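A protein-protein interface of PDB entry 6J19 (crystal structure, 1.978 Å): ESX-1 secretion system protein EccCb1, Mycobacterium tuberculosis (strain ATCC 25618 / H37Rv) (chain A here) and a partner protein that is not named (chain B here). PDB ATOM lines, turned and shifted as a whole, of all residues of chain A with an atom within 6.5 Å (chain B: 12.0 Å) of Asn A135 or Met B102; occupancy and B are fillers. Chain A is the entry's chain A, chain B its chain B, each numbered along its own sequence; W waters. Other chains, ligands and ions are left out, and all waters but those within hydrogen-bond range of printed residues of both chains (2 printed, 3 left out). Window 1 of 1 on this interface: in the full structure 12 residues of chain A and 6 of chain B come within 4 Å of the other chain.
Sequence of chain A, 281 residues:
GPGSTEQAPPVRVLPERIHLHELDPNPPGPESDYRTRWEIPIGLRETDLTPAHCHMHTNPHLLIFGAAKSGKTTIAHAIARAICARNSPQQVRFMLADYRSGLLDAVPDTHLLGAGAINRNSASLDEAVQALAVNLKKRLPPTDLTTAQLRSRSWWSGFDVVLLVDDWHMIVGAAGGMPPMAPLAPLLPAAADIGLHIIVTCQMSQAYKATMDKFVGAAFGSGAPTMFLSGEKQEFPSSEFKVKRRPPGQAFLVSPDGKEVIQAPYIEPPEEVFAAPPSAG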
ATOM      1  N   ARG A  93     -26.971 -21.368   2.955  1.00  0.00           N
ATOM      2  CA  ARG A  93     -25.948 -22.039   2.164  1.00  0.00           C
ATOM      3  C   ARG A  93     -24.600 -21.429   2.523  1.00  0.00           C
ATOM      4  O   ARG A  93     -24.521 -20.254   2.886  1.00  0.00           O
ATOM      5  CB  ARG A  93     -26.178 -21.900   0.648  1.00  0.00           C
ATOM      6  CG  ARG A  93     -27.427 -22.604   0.111  1.00  0.00           C
ATOM      7  CD  ARG A  93     -27.375 -24.115   0.301  1.00  0.00           C
ATOM      8  NE  ARG A  93     -28.613 -24.708  -0.196  1.00  0.00           N
ATOM      9  CZ  ARG A  93     -28.686 -25.611  -1.168  1.00  0.00           C
ATOM     10  NH1 ARG A  93     -27.580 -26.066  -1.743  1.00  0.00           N
ATOM     11  NH2 ARG A  93     -29.870 -26.074  -1.553  1.00  0.00           N
ATOM     12  N   MET A  95     -20.519 -20.618   1.528  1.00  0.00           N
ATOM     13  CA  MET A  95     -19.373 -20.542   0.634  1.00  0.00           C
ATOM     14  C   MET A  95     -18.112 -20.459   1.487  1.00  0.00           C
ATOM     15  O   MET A  95     -18.033 -19.634   2.403  1.00  0.00           O
ATOM     16  CB  MET A  95     -19.456 -19.338  -0.300  1.00  0.00           C
ATOM     17  CG  MET A  95     -18.164 -19.181  -1.134  1.00  0.00           C
ATOM     18  SD  MET A  95     -18.199 -17.811  -2.307  1.00  0.00           S
ATOM     19  CE  MET A  95     -19.467 -18.362  -3.456  1.00  0.00           C
ATOM     20  N   LEU A 113     -23.295 -24.120  -0.793  1.00  0.00           N
ATOM     21  CA  LEU A 113     -23.818 -23.487  -1.994  1.00  0.00           C
ATOM     22  C   LEU A 113     -23.716 -24.444  -3.181  1.00  0.00           C
ATOM     23  O   LEU A 113     -22.777 -25.235  -3.283  1.00  0.00           O
ATOM     24  CB  LEU A 113     -23.043 -22.197  -2.271  1.00  0.00           C
ATOM     25  CG  LEU A 113     -23.642 -21.211  -3.268  1.00  0.00           C
ATOM     26  CD1 LEU A 113     -25.026 -20.702  -2.798  1.00  0.00           C
ATOM     27  CD2 LEU A 113     -22.668 -20.059  -3.468  1.00  0.00           C
ATOM     28  N   GLY A 114     -24.698 -24.366  -4.087  1.00  0.00           N
ATOM     29  CA  GLY A 114     -24.773 -25.322  -5.187  1.00  0.00           C
ATOM     30  C   GLY A 114     -23.585 -25.291  -6.134  1.00  0.00           C
ATOM     31  O   GLY A 114     -23.288 -26.289  -6.802  1.00  0.00           O
ATOM     32  N   ALA A 115     -22.897 -24.157  -6.227  1.00  0.00           N
ATOM     33  CA  ALA A 115     -21.679 -24.079  -7.024  1.00  0.00           C
ATOM     34  C   ALA A 115     -20.761 -23.045  -6.392  1.00  0.00           C
ATOM     35  O   ALA A 115     -21.205 -22.170  -5.643  1.00  0.00           O
ATOM     36  CB  ALA A 115     -21.964 -23.730  -8.490  1.00  0.00           C
ATOM     37  N   GLY A 116     -19.465 -23.179  -6.672  1.00  0.00           N
ATOM     38  CA  GLY A 116     -18.485 -22.255  -6.122  1.00  0.00           C
ATOM     39  C   GLY A 116     -18.315 -22.325  -4.620  1.00  0.00           C
ATOM     40  O   GLY A 116     -17.894 -21.339  -4.004  1.00  0.00           O
ATOM     41  N   ALA A 128     -15.524 -17.411  -7.656  1.00  0.00           N
ATOM     42  CA  ALA A 128     -16.711 -17.729  -6.870  1.00  0.00           C
ATOM     43  C   ALA A 128     -17.357 -16.469  -6.304  1.00  0.00           C
ATOM     44  O   ALA A 128     -18.586 -16.340  -6.310  1.00  0.00           O
ATOM     45  CB  ALA A 128     -16.348 -18.710  -5.750  1.00  0.00           C
ATOM     46  N   GLN A 130     -17.171 -13.337  -7.352  1.00  0.00           N
ATOM     47  CA  GLN A 130     -17.746 -12.584  -8.435  1.00  0.00           C
ATOM     48  C   GLN A 130     -19.144 -13.133  -8.749  1.00  0.00           C
ATOM     49  O   GLN A 130     -20.043 -12.410  -8.813  1.00  0.00           O
ATOM     50  CB  GLN A 130     -16.855 -12.641  -9.660  1.00  0.00           C
ATOM     51  CG  GLN A 130     -16.994 -11.456 -10.555  1.00  0.00           C
ATOM     52  CD  GLN A 130     -15.712 -11.125 -11.318  1.00  0.00           C
ATOM     53  OE1 GLN A 130     -15.774 -10.598 -12.400  1.00  0.00           O
ATOM     54  NE2 GLN A 130     -14.562 -11.444 -10.749  1.00  0.00           N
ATOM     55  N   ALA A 131     -19.273 -14.433  -8.901  1.00  0.00           N
ATOM     56  CA  ALA A 131     -20.578 -15.034  -9.175  1.00  0.00           C
ATOM     57  C   ALA A 131     -21.556 -14.843  -8.015  1.00  0.00           C
ATOM     58  O   ALA A 131     -22.762 -14.648  -8.236  1.00  0.00           O
ATOM     59  CB  ALA A 131     -20.410 -16.520  -9.471  1.00  0.00           C
ATOM     60  N   LEU A 132     -21.066 -14.941  -6.772  1.00  0.00           N
ATOM     61  CA  LEU A 132     -21.931 -14.697  -5.620  1.00  0.00           C
ATOM     62  C   LEU A 132     -22.475 -13.279  -5.643  1.00  0.00           C
ATOM     63  O   LEU A 132     -23.674 -13.059  -5.428  1.00  0.00           O
ATOM     64  CB  LEU A 132     -21.170 -14.969  -4.323  1.00  0.00           C
ATOM     65  CG  LEU A 132     -21.900 -14.712  -3.001  1.00  0.00           C
ATOM     66  CD1 LEU A 132     -23.173 -15.567  -2.884  1.00  0.00           C
ATOM     67  CD2 LEU A 132     -20.960 -14.982  -1.810  1.00  0.00           C
ATOM     68  N   ALA A 133     -21.604 -12.310  -5.932  1.00  0.00           N
ATOM     69  CA  ALA A 133     -22.018 -10.916  -5.970  1.00  0.00           C
ATOM     70  C   ALA A 133     -23.109 -10.691  -7.018  1.00  0.00           C
ATOM     71  O   ALA A 133     -24.050  -9.919  -6.788  1.00  0.00           O
ATOM     72  CB  ALA A 133     -20.794 -10.029  -6.232  1.00  0.00           C
ATOM     73  N   VAL A 134     -23.012 -11.370  -8.168  1.00  0.00           N
ATOM     74  CA  VAL A 134     -24.044 -11.237  -9.199  1.00  0.00           C
ATOM     75  C   VAL A 134     -25.409 -11.631  -8.640  1.00  0.00           C
ATOM     76  O   VAL A 134     -26.407 -10.924  -8.832  1.00  0.00           O
ATOM     77  CB  VAL A 134     -23.675 -12.073 -10.443  1.00  0.00           C
ATOM     78  CG1 VAL A 134     -24.875 -12.183 -11.407  1.00  0.00           C
ATOM     79  CG2 VAL A 134     -22.481 -11.472 -11.149  1.00  0.00           C
ATOM     80  N   ASN A 135     -25.468 -12.750  -7.915  1.00  0.00           N
ATOM     81  CA  ASN A 135     -26.728 -13.206  -7.335  1.00  0.00           C
ATOM     82  C   ASN A 135     -27.190 -12.295  -6.204  1.00  0.00           C
ATOM     83  O   ASN A 135     -28.379 -11.953  -6.123  1.00  0.00           O
ATOM     84  CB  ASN A 135     -26.584 -14.637  -6.826  1.00  0.00           C
ATOM     85  CG  ASN A 135     -26.540 -15.658  -7.949  1.00  0.00           C
ATOM     86  OD1 ASN A 135     -27.555 -15.934  -8.586  1.00  0.00           O
ATOM     87  ND2 ASN A 135     -25.363 -16.245  -8.180  1.00  0.00           N
ATOM     88  N   LEU A 136     -26.266 -11.900  -5.317  1.00  0.00           N
ATOM     89  CA  LEU A 136     -26.639 -11.096  -4.152  1.00  0.00           C
ATOM     90  C   LEU A 136     -27.091  -9.698  -4.554  1.00  0.00           C
ATOM     91  O   LEU A 136     -27.955  -9.107  -3.891  1.00  0.00           O
ATOM     92  CB  LEU A 136     -25.467 -11.014  -3.169  1.00  0.00           C
ATOM     93  CG  LEU A 136     -25.159 -12.300  -2.382  1.00  0.00           C
ATOM     94  CD1 LEU A 136     -24.073 -12.068  -1.344  1.00  0.00           C
ATOM     95  CD2 LEU A 136     -26.400 -12.863  -1.723  1.00  0.00           C
ATOM     96  N   LYS A 137     -26.514  -9.151  -5.631  1.00  0.00           N
ATOM     97  CA  LYS A 137     -26.923  -7.834  -6.107  1.00  0.00           C
ATOM     98  C   LYS A 137     -28.400  -7.813  -6.495  1.00  0.00           C
ATOM     99  O   LYS A 137     -29.083  -6.800  -6.299  1.00  0.00           O
ATOM    100  CB  LYS A 137     -26.054  -7.423  -7.296  1.00  0.00           C
ATOM    101  CG  LYS A 137     -26.264  -6.011  -7.779  1.00  0.00           C
ATOM    102  CD  LYS A 137     -25.139  -5.599  -8.729  1.00  0.00           C
ATOM    103  CE  LYS A 137     -25.363  -4.200  -9.281  1.00  0.00           C
ATOM    104  NZ  LYS A 137     -24.121  -3.640  -9.891  1.00  0.00           N
ATOM    105  N   LYS A 138     -28.917  -8.917  -7.030  1.00  0.00           N
ATOM    106  CA  LYS A 138     -30.324  -8.935  -7.412  1.00  0.00           C
ATOM    107  C   LYS A 138     -31.266  -8.870  -6.215  1.00  0.00           C
ATOM    108  O   LYS A 138     -32.448  -8.575  -6.399  1.00  0.00           O
ATOM    109  CB  LYS A 138     -30.627 -10.175  -8.240  1.00  0.00           C
ATOM    110  CG  LYS A 138     -29.897 -10.198  -9.577  1.00  0.00           C
ATOM    111  CD  LYS A 138     -30.424 -11.310 -10.451  1.00  0.00           C
ATOM    112  CE  LYS A 138     -29.303 -12.196 -10.934  1.00  0.00           C
ATOM    113  NZ  LYS A 138     -29.834 -13.490 -11.438  1.00  0.00           N
ATOM    114  N   ARG A 139     -30.773  -9.110  -5.006  1.00  0.00           N
ATOM    115  CA  ARG A 139     -31.569  -9.023  -3.789  1.00  0.00           C
ATOM    116  C   ARG A 139     -31.588  -7.629  -3.183  1.00  0.00           C
ATOM    117  O   ARG A 139     -32.272  -7.429  -2.172  1.00  0.00           O
ATOM    118  CB  ARG A 139     -31.033  -9.989  -2.736  1.00  0.00           C
ATOM    119  CG  ARG A 139     -31.115 -11.459  -3.082  1.00  0.00           C
ATOM    120  CD  ARG A 139     -30.738 -12.277  -1.852  1.00  0.00           C
ATOM    121  NE  ARG A 139     -31.041 -13.691  -2.018  1.00  0.00           N
ATOM    122  CZ  ARG A 139     -30.623 -14.649  -1.199  1.00  0.00           C
ATOM    123  NH1 ARG A 139     -29.880 -14.337  -0.141  1.00  0.00           N
ATOM    124  NH2 ARG A 139     -30.982 -15.913  -1.406  1.00  0.00           N
ATOM    125  N   LEU A 140     -30.820  -6.686  -3.722  1.00  0.00           N
ATOM    126  CA  LEU A 140     -30.819  -5.348  -3.154  1.00  0.00           C
ATOM    127  C   LEU A 140     -32.248  -4.807  -3.158  1.00  0.00           C
ATOM    128  O   LEU A 140     -32.989  -5.027  -4.119  1.00  0.00           O
ATOM    129  CB  LEU A 140     -29.891  -4.417  -3.937  1.00  0.00           C
ATOM    130  CG  LEU A 140     -28.370  -4.627  -3.812  1.00  0.00           C
ATOM    131  CD1 LEU A 140     -27.628  -3.782  -4.838  1.00  0.00           C
ATOM    132  CD2 LEU A 140     -27.869  -4.305  -2.413  1.00  0.00           C
ATOM    133  N   PHE A 159     -32.361 -18.852   0.618  1.00  0.00           N
ATOM    134  CA  PHE A 159     -31.453 -19.031   1.743  1.00  0.00           C
ATOM    135  C   PHE A 159     -30.639 -17.766   1.998  1.00  0.00           C
ATOM    136  O   PHE A 159     -30.349 -16.989   1.079  1.00  0.00           O
ATOM    137  CB  PHE A 159     -30.505 -20.212   1.493  1.00  0.00           C
ATOM    138  CG  PHE A 159     -29.962 -20.268   0.081  1.00  0.00           C
ATOM    139  CD1 PHE A 159     -28.935 -19.417  -0.319  1.00  0.00           C
ATOM    140  CD2 PHE A 159     -30.489 -21.162  -0.852  1.00  0.00           C
ATOM    141  CE1 PHE A 159     -28.432 -19.456  -1.625  1.00  0.00           C
ATOM    142  CE2 PHE A 159     -29.989 -21.214  -2.158  1.00  0.00           C
ATOM    143  CZ  PHE A 159     -28.962 -20.358  -2.547  1.00  0.00           C
ATOM    144  N   LEU A 187     -21.731  -4.458  -1.798  1.00  0.00           N
ATOM    145  CA  LEU A 187     -22.916  -5.101  -1.250  1.00  0.00           C
ATOM    146  C   LEU A 187     -22.912  -5.170   0.270  1.00  0.00           C
ATOM    147  O   LEU A 187     -23.973  -5.397   0.865  1.00  0.00           O
ATOM    148  CB  LEU A 187     -23.054  -6.515  -1.831  1.00  0.00           C
ATOM    149  CG  LEU A 187     -23.078  -6.510  -3.369  1.00  0.00           C
ATOM    150  CD1 LEU A 187     -23.076  -7.920  -3.926  1.00  0.00           C
ATOM    151  CD2 LEU A 187     -24.270  -5.717  -3.891  1.00  0.00           C
ATOM    152  N   GLU B  93     -23.384 -16.550 -22.384  1.00  0.00           N
ATOM    153  CA  GLU B  93     -23.710 -17.715 -21.570  1.00  0.00           C
ATOM    154  C   GLU B  93     -22.518 -18.151 -20.731  1.00  0.00           C
ATOM    155  O   GLU B  93     -22.688 -18.697 -19.629  1.00  0.00           O
ATOM    156  CB  GLU B  93     -24.166 -18.857 -22.468  1.00  0.00           C
ATOM    157  CG  GLU B  93     -24.937 -19.978 -21.783  1.00  0.00           C
ATOM    158  CD  GLU B  93     -24.832 -21.298 -22.530  1.00  0.00           C
ATOM    159  OE1 GLU B  93     -25.453 -22.288 -22.089  1.00  0.00           O
ATOM    160  OE2 GLU B  93     -24.122 -21.342 -23.558  1.00  0.00           O
ATOM    161  N   GLN B  94     -21.299 -17.921 -21.229  1.00  0.00           N
ATOM    162  CA  GLN B  94     -20.096 -18.383 -20.549  1.00  0.00           C
ATOM    163  C   GLN B  94     -19.816 -17.574 -19.291  1.00  0.00           C
ATOM    164  O   GLN B  94     -19.392 -18.132 -18.270  1.00  0.00           O
ATOM    165  CB  GLN B  94     -18.915 -18.315 -21.516  1.00  0.00           C
ATOM    166  CG  GLN B  94     -17.553 -18.307 -20.863  1.00  0.00           C
ATOM    167  CD  GLN B  94     -17.118 -19.687 -20.451  1.00  0.00           C
ATOM    168  OE1 GLN B  94     -16.387 -20.357 -21.178  1.00  0.00           O
ATOM    169  NE2 GLN B  94     -17.560 -20.125 -19.279  1.00  0.00           N
ATOM    170  N   GLN B  95     -20.060 -16.263 -19.332  1.00  0.00           N
ATOM    171  CA  GLN B  95     -19.769 -15.413 -18.182  1.00  0.00           C
ATOM    172  C   GLN B  95     -20.719 -15.653 -17.016  1.00  0.00           C
ATOM    173  O   GLN B  95     -20.350 -15.390 -15.867  1.00  0.00           O
ATOM    174  CB  GLN B  95     -19.812 -13.946 -18.602  1.00  0.00           C
ATOM    175  CG  GLN B  95     -18.966 -13.643 -19.825  1.00  0.00           C
ATOM    176  CD  GLN B  95     -18.886 -12.163 -20.112  1.00  0.00           C
ATOM    177  OE1 GLN B  95     -19.661 -11.374 -19.572  1.00  0.00           O
ATOM    178  NE2 GLN B  95     -17.945 -11.774 -20.966  1.00  0.00           N
ATOM    179  N   GLN B  96     -21.927 -16.144 -17.285  1.00  0.00           N
ATOM    180  CA  GLN B  96     -22.907 -16.443 -16.251  1.00  0.00           C
ATOM    181  C   GLN B  96     -23.002 -17.934 -15.949  1.00  0.00           C
ATOM    182  O   GLN B  96     -23.912 -18.353 -15.225  1.00  0.00           O
ATOM    183  CB  GLN B  96     -24.281 -15.903 -16.658  1.00  0.00           C
ATOM    184  CG  GLN B  96     -24.686 -14.651 -15.898  1.00  0.00           C
ATOM    185  CD  GLN B  96     -25.984 -14.049 -16.392  1.00  0.00           C
ATOM    186  OE1 GLN B  96     -26.670 -14.628 -17.236  1.00  0.00           O
ATOM    187  NE2 GLN B  96     -26.329 -12.879 -15.865  1.00  0.00           N
ATOM    188  N   ALA B  97     -22.077 -18.738 -16.482  1.00  0.00           N
ATOM    189  CA  ALA B  97     -22.161 -20.185 -16.330  1.00  0.00           C
ATOM    190  C   ALA B  97     -22.009 -20.606 -14.876  1.00  0.00           C
ATOM    191  O   ALA B  97     -22.530 -21.653 -14.479  1.00  0.00           O
ATOM    192  CB  ALA B  97     -21.100 -20.863 -17.201  1.00  0.00           C
ATOM    193  N   LEU B  98     -21.311 -19.804 -14.070  1.00  0.00           N
ATOM    194  CA  LEU B  98     -21.187 -20.070 -12.638  1.00  0.00           C
ATOM    195  C   LEU B  98     -22.323 -19.440 -11.831  1.00  0.00           C
ATOM    196  O   LEU B  98     -23.002 -20.131 -11.060  1.00  0.00           O
ATOM    197  CB  LEU B  98     -19.838 -19.568 -12.129  1.00  0.00           C
ATOM    198  CG  LEU B  98     -19.572 -19.786 -10.635  1.00  0.00           C
ATOM    199  CD1 LEU B  98     -19.875 -21.213 -10.235  1.00  0.00           C
ATOM    200  CD2 LEU B  98     -18.156 -19.404 -10.243  1.00  0.00           C
ATOM    201  N   SER B  99     -22.551 -18.133 -11.989  1.00  0.00           N
ATOM    202  CA  SER B  99     -23.554 -17.452 -11.174  1.00  0.00           C
ATOM    203  C   SER B  99     -24.956 -18.031 -11.372  1.00  0.00           C
ATOM    204  O   SER B  99     -25.763 -18.019 -10.437  1.00  0.00           O
ATOM    205  CB  SER B  99     -23.556 -15.956 -11.484  1.00  0.00           C
ATOM    206  OG  SER B  99     -23.908 -15.734 -12.840  1.00  0.00           O
ATOM    207  N   SER B 100     -25.266 -18.550 -12.562  1.00  0.00           N
ATOM    208  CA  SER B 100     -26.601 -19.088 -12.818  1.00  0.00           C
ATOM    209  C   SER B 100     -26.830 -20.459 -12.194  1.00  0.00           C
ATOM    210  O   SER B 100     -27.963 -20.953 -12.228  1.00  0.00           O
ATOM    211  CB  SER B 100     -26.863 -19.164 -14.328  1.00  0.00           C
ATOM    212  OG  SER B 100     -25.978 -20.073 -14.963  1.00  0.00           O
ATOM    213  N   GLN B 101     -25.799 -21.079 -11.614  1.00  0.00           N
ATOM    214  CA  GLN B 101     -25.893 -22.439 -11.096  1.00  0.00           C
ATOM    215  C   GLN B 101     -25.694 -22.496  -9.585  1.00  0.00           C
ATOM    216  O   GLN B 101     -25.402 -23.563  -9.039  1.00  0.00           O
ATOM    217  CB  GLN B 101     -24.880 -23.347 -11.791  1.00  0.00           C
ATOM    218  CG  GLN B 101     -25.185 -23.610 -13.252  1.00  0.00           C
ATOM    219  CD  GLN B 101     -26.475 -24.384 -13.435  1.00  0.00           C
ATOM    220  OE1 GLN B 101     -26.747 -25.339 -12.711  1.00  0.00           O
ATOM    221  NE2 GLN B 101     -27.277 -23.971 -14.404  1.00  0.00           N
ATOM    222  N   MET B 102     -25.830 -21.379  -8.888  1.00  0.00           N
ATOM    223  CA  MET B 102     -25.614 -21.408  -7.447  1.00  0.00           C
ATOM    224  C   MET B 102     -26.887 -21.659  -6.649  1.00  0.00           C
ATOM    225  O   MET B 102     -26.828 -21.681  -5.415  1.00  0.00           O
ATOM    226  CB  MET B 102     -24.972 -20.109  -6.981  1.00  0.00           C
ATOM    227  CG  MET B 102     -23.462 -20.197  -6.948  1.00  0.00           C
ATOM    228  SD  MET B 102     -22.705 -18.633  -7.374  1.00  0.00           S
ATOM    229  CE  MET B 102     -23.287 -17.591  -6.137  1.00  0.00           C
ATOM    230  N   GLY B 103     -28.026 -21.846  -7.311  1.00  0.00           N
ATOM    231  CA  GLY B 103     -29.236 -22.246  -6.620  1.00  0.00           C
ATOM    232  C   GLY B 103     -30.103 -21.122  -6.105  1.00  0.00           C
ATOM    233  O   GLY B 103     -31.054 -21.391  -5.359  1.00  0.00           O
ATOM    234  N   PHE B 104     -29.812 -19.876  -6.465  1.00  0.00           N
ATOM    235  CA  PHE B 104     -30.668 -18.770  -6.046  1.00  0.00           C
ATOM    236  C   PHE B 104     -32.009 -18.823  -6.780  1.00  0.00           C
ATOM    237  O   PHE B 104     -32.945 -18.125  -6.396  1.00  0.00           O
ATOM    238  CB  PHE B 104     -29.990 -17.424  -6.299  1.00  0.00           C
ATOM    239  CG  PHE B 104     -28.832 -17.138  -5.381  1.00  0.00           C
ATOM    240  CD1 PHE B 104     -27.602 -17.731  -5.597  1.00  0.00           C
ATOM    241  CD2 PHE B 104     -28.973 -16.270  -4.309  1.00  0.00           C
ATOM    242  CE1 PHE B 104     -26.527 -17.471  -4.761  1.00  0.00           C
ATOM    243  CE2 PHE B 104     -27.899 -15.998  -3.465  1.00  0.00           C
ATOM    244  CZ  PHE B 104     -26.679 -16.601  -3.696  1.00  0.00           C
HETATM  245  O   HOH W   1     -27.899 -15.568 -11.301  1.00  0.00           O
HETATM  246  O   HOH W   2     -27.175 -23.550  -3.584  1.00  0.00           O
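Water W2 lies within hydrogen-bond range of the backbone carbonyl oxygen of Met B102 (2.6 Å), the backbone NH of Gly A114 (2.7 Å) and the guanidinium group of Arg A93 (3.1 Å).
Water W1 lies within hydrogen-bond range of OD1 of Asn A135 (2.8 Å), NZ of Lys A138 (2.8 Å) and O of Ser B99 (3.4 Å).
Of the 20 printed residues of chain A, 10 touch a printed residue of chain B.
Printed residues of chain A that touch a printed residue of chain B: Leu A113, Gly A114, Ala A115, Ala A131, Leu A132, Val A134, Asn A135, Leu A136, Arg A139 and Phe A159.
Hydrophobic or aromatic side chains of chain B that line the printed part of chain A: Leu B98, Met B102 and Phe B104.
The side-chain amide nitrogen (ND2) of Asn A135 sits at hydrogen-bond distance from the backbone carbonyl oxygen (O) of Ser B99.
The side-chain amide nitrogen (ND2) of Asn A135 sits close to the side-chain sulfur (SD) of Met B102 (3.7 Å).
O of Ala A131 is in hydrogen-bond range of ND2 of Asn A135, 3.1 Å away.
NH2 of Arg A139 sits at hydrogen-bond distance from O of Phe A159, at 2.8 Å.
Of the printed residues of chain B, Leu A113 touches Met B102 (3.3 Å).
Of chain B, only Gln B101 (3.8 Å) and Met B102 (3.7 Å) come within 4 Å of Gly A114.
Ala A115 touches three residues of chain B.
No residue of chain B comes within 4 Å of Gly A116.
No residue of chain B comes within 4 Å of Ala A128.
Ala A131 touches three residues of chain B.
Val A134 touches one residue of chain B.
Leu A136 touches just one residue of chain B: Phe B104 (3.9 Å).
Lys A138 touches none of the printed residues of chain B.
Of the printed residues of chain B, Arg A139 touches Phe B104 (3.5 Å).
Of the printed residues of chain A, Gln B101 touches Gly A114 and Ala A115.
Of the printed residues of chain B, Phe A159 touches Met B102, Gly B103 and Phe B104.
Of the printed residues of chain A, Ser B99 touches Ala A131, Val A134 and Asn A135.
Met A95 touches none of the printed residues of chain B.
The nearest printed residue of chain A that does not touch Ser B99 is Leu A132 (5.4 Å).
Among the printed residues, merely in contact across the chains: Leu A132 with Met B102 (3.2 Å), Ala A115 with Met B102 (3.3 Å), Asn A135 with Phe B104 (3.3 Å), Leu A113 with Met B102 (3.3 Å), Phe A159 with Gly B103 (3.4 Å), Ala A115 with Gln B101 (3.5 Å), Arg A139 with Phe B104 (3.5 Å), Ala A131 with Leu B98 (3.6 Å), Ala A131 with Ser B99 (3.6 Å), Ala A131 with Met B102 (3.7 Å), Gly A114 with Met B102 (3.7 Å), Ala A115 with Leu B98 (3.7 Å), Leu A132 with Phe B104 (3.7 Å), Phe A159 with Met B102 (3.8 Å), Gly A114 with Gln B101 (3.8 Å), Leu A136 with Phe B104 (3.9 Å), Phe A159 with Phe B104 (3.9 Å) and Val A134 with Ser B99 (3.9 Å).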
